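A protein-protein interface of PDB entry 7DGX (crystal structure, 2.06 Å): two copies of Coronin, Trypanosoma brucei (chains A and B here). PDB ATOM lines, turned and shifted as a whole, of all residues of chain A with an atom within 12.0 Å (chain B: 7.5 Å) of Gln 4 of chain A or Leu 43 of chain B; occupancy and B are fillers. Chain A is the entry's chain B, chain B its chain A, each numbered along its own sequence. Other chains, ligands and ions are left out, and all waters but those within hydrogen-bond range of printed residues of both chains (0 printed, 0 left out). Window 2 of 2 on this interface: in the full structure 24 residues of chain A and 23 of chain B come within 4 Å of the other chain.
N of Leu 5 of chain A sits at hydrogen-bond distance from OG of Ser 3 of chain A (2.9 Å).
CB of Gln 4 of chain A touches CD1 of Leu 43 of chain B (3.8 Å).
Leu 5 of chain A touches Leu 43 of chain B.
CD2 of Leu 8 of chain A touches CB of Lys 39 of chain B (3.8 Å).
Leu 8 of chain A touches Ile 40 of chain B (CB to CG1, 3.8 Å).
CD2 of Leu 12 of chain A touches CD1 of Ile 37 of chain B, 3.8 Å away.
Ile 40 of chain B touches Leu 12 of chain A (CD1 to CD2, 3.9 Å).
Gln 4 of chain A touches just one residue of chain B: Leu 43 (3.8 Å).
Printed residues of chain B within 4 Å of Leu 8 of chain A: Lys 39 and Ile 40.
Ala 9 of chain A touches none of the printed residues of chain B.
Printed residues of chain A within 4 Å of Ile 37 of chain B: Leu 12.
Printed residues of chain A within 4 Å of Lys 39 of chain B: Leu 8.
No residue of chain A comes within 4 Å of Ala 42 of chain B.
Leu 43 of chain B touches just these residues of chain A: Gln 4 (3.8 Å) and Leu 5 (3.9 Å).
No residue of chain A comes within 4 Å of Ala 44 of chain B.
No residue of chain A comes within 4 Å of Leu 45 of chain B.
The nearest residue of chain A that does not touch Leu 43 of chain B is Leu 8 of chain A (4.1 Å).
Hydrophobic or aromatic side chains of chain B within 4 Å of the printed part of chain A: Ile 37, Ile 40 and Leu 43.
Along chain B the printed residues that touch a printed residue of chain A span positions 37 to 43.
Printed residues of chain A that touch a printed residue of chain B: Gln 4, Leu 5, Leu 8 and Leu 12.
Hydrophobic or aromatic side chains of chain A within 4 Å of the printed part of chain B: Leu 5, Leu 8 and Leu 12.
Along chain A the printed residues that touch a printed residue of chain B span positions 4 to 12.
Among the printed residues, 6 pairs touch across the chains.
No position is printed for both chains.
Of the 6 pairs that touch across the chains among the printed residues, none has its exchanged pair printed and touching as well.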
ATOM      1  N   SER A   3      -5.578 -20.092  -3.411  1.00  0.00           N
ATOM      2  CA  SER A   3      -6.723 -19.280  -3.013  1.00  0.00           C
ATOM      3  C   SER A   3      -6.419 -18.480  -1.752  1.00  0.00           C
ATOM      4  O   SER A   3      -5.489 -18.799  -1.012  1.00  0.00           O
ATOM      5  CB  SER A   3      -7.953 -20.162  -2.788  1.00  0.00           C
ATOM      6  OG  SER A   3      -8.829 -19.587  -1.835  1.00  0.00           O
ATOM      7  N   GLN A   4      -7.214 -17.433  -1.514  1.00  0.00           N
ATOM      8  CA  GLN A   4      -7.041 -16.637  -0.303  1.00  0.00           C
ATOM      9  C   GLN A   4      -7.322 -17.456   0.949  1.00  0.00           C
ATOM     10  O   GLN A   4      -6.810 -17.138   2.028  1.00  0.00           O
ATOM     11  CB  GLN A   4      -7.948 -15.408  -0.348  1.00  0.00           C
ATOM     12  N   LEU A   5      -8.073 -18.525   0.800  1.00  0.00           N
ATOM     13  CA  LEU A   5      -8.404 -19.381   1.948  1.00  0.00           C
ATOM     14  C   LEU A   5      -7.137 -20.074   2.434  1.00  0.00           C
ATOM     15  O   LEU A   5      -6.977 -20.257   3.600  1.00  0.00           O
ATOM     16  CB  LEU A   5      -9.439 -20.389   1.465  1.00  0.00           C
ATOM     17  CG  LEU A   5     -10.670 -20.562   2.339  1.00  0.00           C
ATOM     18  CD1 LEU A   5     -11.051 -19.262   2.993  1.00  0.00           C
ATOM     19  CD2 LEU A   5     -11.821 -21.088   1.535  1.00  0.00           C
ATOM     20  N   LEU A   6      -6.270 -20.460   1.526  1.00  0.00           N
ATOM     21  CA  LEU A   6      -5.034 -21.132   1.914  1.00  0.00           C
ATOM     22  C   LEU A   6      -4.125 -20.205   2.711  1.00  0.00           C
ATOM     23  O   LEU A   6      -3.515 -20.624   3.702  1.00  0.00           O
ATOM     24  CB  LEU A   6      -4.309 -21.655   0.675  1.00  0.00           C
ATOM     25  CG  LEU A   6      -2.920 -22.260   0.894  1.00  0.00           C
ATOM     26  CD1 LEU A   6      -2.995 -23.445   1.842  1.00  0.00           C
ATOM     27  CD2 LEU A   6      -2.297 -22.667  -0.432  1.00  0.00           C
ATOM     28  N   ALA A   7      -4.022 -18.941   2.295  1.00  0.00           N
ATOM     29  CA  ALA A   7      -3.170 -17.996   3.008  1.00  0.00           C
ATOM     30  C   ALA A   7      -3.718 -17.692   4.396  1.00  0.00           C
ATOM     31  O   ALA A   7      -2.960 -17.641   5.371  1.00  0.00           O
ATOM     32  CB  ALA A   7      -3.016 -16.711   2.195  1.00  0.00           C
ATOM     33  N   LEU A   8      -5.034 -17.490   4.508  1.00  0.00           N
ATOM     34  CA  LEU A   8      -5.620 -17.177   5.807  1.00  0.00           C
ATOM     35  C   LEU A   8      -5.571 -18.380   6.742  1.00  0.00           C
ATOM     36  O   LEU A   8      -5.350 -18.224   7.949  1.00  0.00           O
ATOM     37  CB  LEU A   8      -7.057 -16.684   5.630  1.00  0.00           C
ATOM     38  CG  LEU A   8      -7.237 -15.393   4.826  1.00  0.00           C
ATOM     39  CD1 LEU A   8      -8.681 -15.231   4.373  1.00  0.00           C
ATOM     40  CD2 LEU A   8      -6.790 -14.186   5.639  1.00  0.00           C
ATOM     41  N   ALA A   9      -5.772 -19.588   6.207  1.00  0.00           N
ATOM     42  CA  ALA A   9      -5.680 -20.783   7.040  1.00  0.00           C
ATOM     43  C   ALA A   9      -4.251 -21.009   7.521  1.00  0.00           C
ATOM     44  O   ALA A   9      -4.033 -21.427   8.664  1.00  0.00           O
ATOM     45  CB  ALA A   9      -6.189 -22.003   6.276  1.00  0.00           C
ATOM     46  N   SER A  10      -3.266 -20.742   6.660  1.00  0.00           N
ATOM     47  CA  SER A  10      -1.872 -20.853   7.078  1.00  0.00           C
ATOM     48  C   SER A  10      -1.534 -19.812   8.137  1.00  0.00           C
ATOM     49  O   SER A  10      -0.860 -20.119   9.128  1.00  0.00           O
ATOM     50  CB  SER A  10      -0.948 -20.708   5.868  1.00  0.00           C
ATOM     51  OG  SER A  10       0.380 -20.425   6.273  1.00  0.00           O
ATOM     52  N   LEU A  11      -1.997 -18.574   7.946  1.00  0.00           N
ATOM     53  CA  LEU A  11      -1.751 -17.532   8.938  1.00  0.00           C
ATOM     54  C   LEU A  11      -2.464 -17.842  10.248  1.00  0.00           C
ATOM     55  O   LEU A  11      -1.916 -17.606  11.331  1.00  0.00           O
ATOM     56  CB  LEU A  11      -2.197 -16.176   8.393  1.00  0.00           C
ATOM     57  CG  LEU A  11      -2.138 -15.004   9.376  1.00  0.00           C
ATOM     58  CD1 LEU A  11      -0.697 -14.681   9.740  1.00  0.00           C
ATOM     59  CD2 LEU A  11      -2.843 -13.782   8.805  1.00  0.00           C
ATOM     60  N   LEU A  12      -3.687 -18.373  10.168  1.00  0.00           N
ATOM     61  CA  LEU A  12      -4.425 -18.719  11.380  1.00  0.00           C
ATOM     62  C   LEU A  12      -3.702 -19.797  12.177  1.00  0.00           C
ATOM     63  O   LEU A  12      -3.603 -19.708  13.407  1.00  0.00           O
ATOM     64  CB  LEU A  12      -5.838 -19.176  11.018  1.00  0.00           C
ATOM     65  CG  LEU A  12      -6.675 -19.780  12.148  1.00  0.00           C
ATOM     66  CD1 LEU A  12      -6.946 -18.744  13.226  1.00  0.00           C
ATOM     67  CD2 LEU A  12      -7.974 -20.351  11.604  1.00  0.00           C
ATOM     68  N   GLY A  13      -3.188 -20.823  11.496  1.00  0.00           N
ATOM     69  CA  GLY A  13      -2.444 -21.860  12.191  1.00  0.00           C
ATOM     70  C   GLY A  13      -1.186 -21.331  12.853  1.00  0.00           C
ATOM     71  O   GLY A  13      -0.844 -21.732  13.968  1.00  0.00           O
ATOM     72  N   GLN A  15      -0.720 -18.136  13.836  1.00  0.00           N
ATOM     73  CA  GLN A  15      -1.121 -17.259  14.929  1.00  0.00           C
ATOM     74  C   GLN A  15      -1.661 -18.056  16.111  1.00  0.00           C
ATOM     75  O   GLN A  15      -1.407 -17.705  17.269  1.00  0.00           O
ATOM     76  CB  GLN A  15      -2.160 -16.252  14.437  1.00  0.00           C
ATOM     77  CG  GLN A  15      -1.597 -15.177  13.519  1.00  0.00           C
ATOM     78  CD  GLN A  15      -2.679 -14.333  12.876  1.00  0.00           C
ATOM     79  OE1 GLN A  15      -3.805 -14.791  12.680  1.00  0.00           O
ATOM     80  NE2 GLN A  15      -2.342 -13.092  12.543  1.00  0.00           N
ATOM     81  N   ILE B  37      -9.810 -14.842  11.733  1.00  0.00           N
ATOM     82  CA  ILE B  37     -11.098 -15.533  11.712  1.00  0.00           C
ATOM     83  C   ILE B  37     -12.140 -14.682  10.999  1.00  0.00           C
ATOM     84  O   ILE B  37     -12.917 -15.179  10.174  1.00  0.00           O
ATOM     85  CB  ILE B  37     -11.540 -15.884  13.144  1.00  0.00           C
ATOM     86  CG1 ILE B  37     -10.640 -16.972  13.736  1.00  0.00           C
ATOM     87  CG2 ILE B  37     -12.999 -16.321  13.164  1.00  0.00           C
ATOM     88  CD1 ILE B  37     -10.845 -18.338  13.124  1.00  0.00           C
ATOM     89  N   ALA B  38     -12.167 -13.382  11.305  1.00  0.00           N
ATOM     90  CA  ALA B  38     -13.117 -12.485  10.656  1.00  0.00           C
ATOM     91  C   ALA B  38     -12.884 -12.411   9.153  1.00  0.00           C
ATOM     92  O   ALA B  38     -13.842 -12.274   8.383  1.00  0.00           O
ATOM     93  CB  ALA B  38     -13.031 -11.090  11.276  1.00  0.00           C
ATOM     94  N   LYS B  39     -11.625 -12.498   8.716  1.00  0.00           N
ATOM     95  CA  LYS B  39     -11.344 -12.513   7.285  1.00  0.00           C
ATOM     96  C   LYS B  39     -11.843 -13.799   6.640  1.00  0.00           C
ATOM     97  O   LYS B  39     -12.365 -13.777   5.519  1.00  0.00           O
ATOM     98  CB  LYS B  39      -9.845 -12.338   7.042  1.00  0.00           C
ATOM     99  CG  LYS B  39      -9.398 -10.889   6.941  1.00  0.00           C
ATOM    100  CD  LYS B  39      -8.140 -10.643   7.756  1.00  0.00           C
ATOM    101  CE  LYS B  39      -7.099  -9.890   6.946  1.00  0.00           C
ATOM    102  NZ  LYS B  39      -5.872  -9.612   7.742  1.00  0.00           N
ATOM    103  N   ILE B  40     -11.690 -14.930   7.333  1.00  0.00           N
ATOM    104  CA  ILE B  40     -12.210 -16.194   6.820  1.00  0.00           C
ATOM    105  C   ILE B  40     -13.732 -16.158   6.763  1.00  0.00           C
ATOM    106  O   ILE B  40     -14.343 -16.626   5.795  1.00  0.00           O
ATOM    107  CB  ILE B  40     -11.702 -17.365   7.681  1.00  0.00           C
ATOM    108  CG1 ILE B  40     -10.179 -17.482   7.585  1.00  0.00           C
ATOM    109  CG2 ILE B  40     -12.368 -18.670   7.264  1.00  0.00           C
ATOM    110  CD1 ILE B  40      -9.587 -18.496   8.541  1.00  0.00           C
ATOM    111  N   LYS B  41     -14.366 -15.595   7.795  1.00  0.00           N
ATOM    112  CA  LYS B  41     -15.822 -15.527   7.828  1.00  0.00           C
ATOM    113  C   LYS B  41     -16.360 -14.631   6.719  1.00  0.00           C
ATOM    114  O   LYS B  41     -17.356 -14.970   6.066  1.00  0.00           O
ATOM    115  CB  LYS B  41     -16.285 -15.033   9.200  1.00  0.00           C
ATOM    116  CG  LYS B  41     -17.674 -14.420   9.225  1.00  0.00           C
ATOM    117  CD  LYS B  41     -18.062 -14.031  10.643  1.00  0.00           C
ATOM    118  CE  LYS B  41     -18.955 -12.802  10.664  1.00  0.00           C
ATOM    119  NZ  LYS B  41     -19.332 -12.422  12.054  1.00  0.00           N
ATOM    120  N   ALA B  42     -15.714 -13.486   6.488  1.00  0.00           N
ATOM    121  CA  ALA B  42     -16.149 -12.595   5.418  1.00  0.00           C
ATOM    122  C   ALA B  42     -16.021 -13.266   4.057  1.00  0.00           C
ATOM    123  O   ALA B  42     -16.874 -13.083   3.181  1.00  0.00           O
ATOM    124  CB  ALA B  42     -15.345 -11.296   5.455  1.00  0.00           C
ATOM    125  N   LEU B  43     -14.956 -14.048   3.860  1.00  0.00           N
ATOM    126  CA  LEU B  43     -14.820 -14.816   2.628  1.00  0.00           C
ATOM    127  C   LEU B  43     -15.919 -15.865   2.515  1.00  0.00           C
ATOM    128  O   LEU B  43     -16.470 -16.087   1.430  1.00  0.00           O
ATOM    129  CB  LEU B  43     -13.441 -15.474   2.572  1.00  0.00           C
ATOM    130  CG  LEU B  43     -12.843 -15.786   1.196  1.00  0.00           C
ATOM    131  CD1 LEU B  43     -11.325 -15.761   1.267  1.00  0.00           C
ATOM    132  CD2 LEU B  43     -13.329 -17.130   0.674  1.00  0.00           C
ATOM    133  N   ALA B  44     -16.254 -16.517   3.631  1.00  0.00           N
ATOM    134  CA  ALA B  44     -17.296 -17.539   3.611  1.00  0.00           C
ATOM    135  C   ALA B  44     -18.661 -16.932   3.311  1.00  0.00           C
ATOM    136  O   ALA B  44     -19.452 -17.509   2.554  1.00  0.00           O
ATOM    137  CB  ALA B  44     -17.321 -18.284   4.945  1.00  0.00           C
ATOM    138  N   LEU B  45     -18.954 -15.766   3.892  1.00  0.00           N
ATOM    139  CA  LEU B  45     -20.250 -15.131   3.669  1.00  0.00           C
ATOM    140  C   LEU B  45     -20.420 -14.682   2.224  1.00  0.00           C
ATOM    141  O   LEU B  45     -21.549 -14.637   1.720  1.00  0.00           O
ATOM    142  CB  LEU B  45     -20.419 -13.941   4.613  1.00  0.00           C
ATOM    143  CG  LEU B  45     -20.812 -14.261   6.057  1.00  0.00           C
ATOM    144  CD1 LEU B  45     -20.740 -13.014   6.924  1.00  0.00           C
ATOM    145  CD2 LEU B  45     -22.202 -14.874   6.109  1.00  0.00           C
ATOM    146  N   GLU B  46     -19.322 -14.349   1.543  1.00  0.00           N
ATOM    147  CA  GLU B  46     -19.420 -13.882   0.164  1.00  0.00           C
ATOM    148  C   GLU B  46     -19.804 -15.015  -0.781  1.00  0.00           C
ATOM    149  O   GLU B  46     -20.656 -14.836  -1.659  1.00  0.00           O
ATOM    150  CB  GLU B  46     -18.098 -13.247  -0.267  1.00  0.00           C
ATOM    151  CG  GLU B  46     -17.999 -12.960  -1.757  1.00  0.00           C
ATOM    152  CD  GLU B  46     -18.057 -11.478  -2.072  1.00  0.00           C
ATOM    153  OE1 GLU B  46     -18.727 -10.736  -1.323  1.00  0.00           O
ATOM    154  OE2 GLU B  46     -17.432 -11.055  -3.066  1.00  0.00           O
ATOM    155  N   HIS B  47     -19.193 -16.185  -0.616  1.00  0.00           N
ATOM    156  CA  HIS B  47     -19.413 -17.315  -1.506  1.00  0.00           C
ATOM    157  C   HIS B  47     -20.561 -18.215  -1.062  1.00  0.00           C
ATOM    158  O   HIS B  47     -20.748 -19.289  -1.640  1.00  0.00           O
ATOM    159  CB  HIS B  47     -18.129 -18.140  -1.635  1.00  0.00           C
ATOM    160  N   HIS B  48     -21.332 -17.804  -0.055  1.00  0.00           N
ATOM    161  CA  HIS B  48     -22.453 -18.597   0.436  1.00  0.00           C
ATOM    162  C   HIS B  48     -23.807 -17.947   0.213  1.00  0.00           C
ATOM    163  O   HIS B  48     -24.785 -18.658  -0.027  1.00  0.00           O
ATOM    164  CB  HIS B  48     -22.285 -18.887   1.933  1.00  0.00           C
ATOM    165  CG  HIS B  48     -23.348 -19.777   2.499  1.00  0.00           C
ATOM    166  ND1 HIS B  48     -24.405 -19.295   3.240  1.00  0.00           N
ATOM    167  CD2 HIS B  48     -23.518 -21.118   2.431  1.00  0.00           C
ATOM    168  CE1 HIS B  48     -25.180 -20.300   3.606  1.00  0.00           C
ATOM    169  NE2 HIS B  48     -24.664 -21.418   3.126  1.00  0.00           N
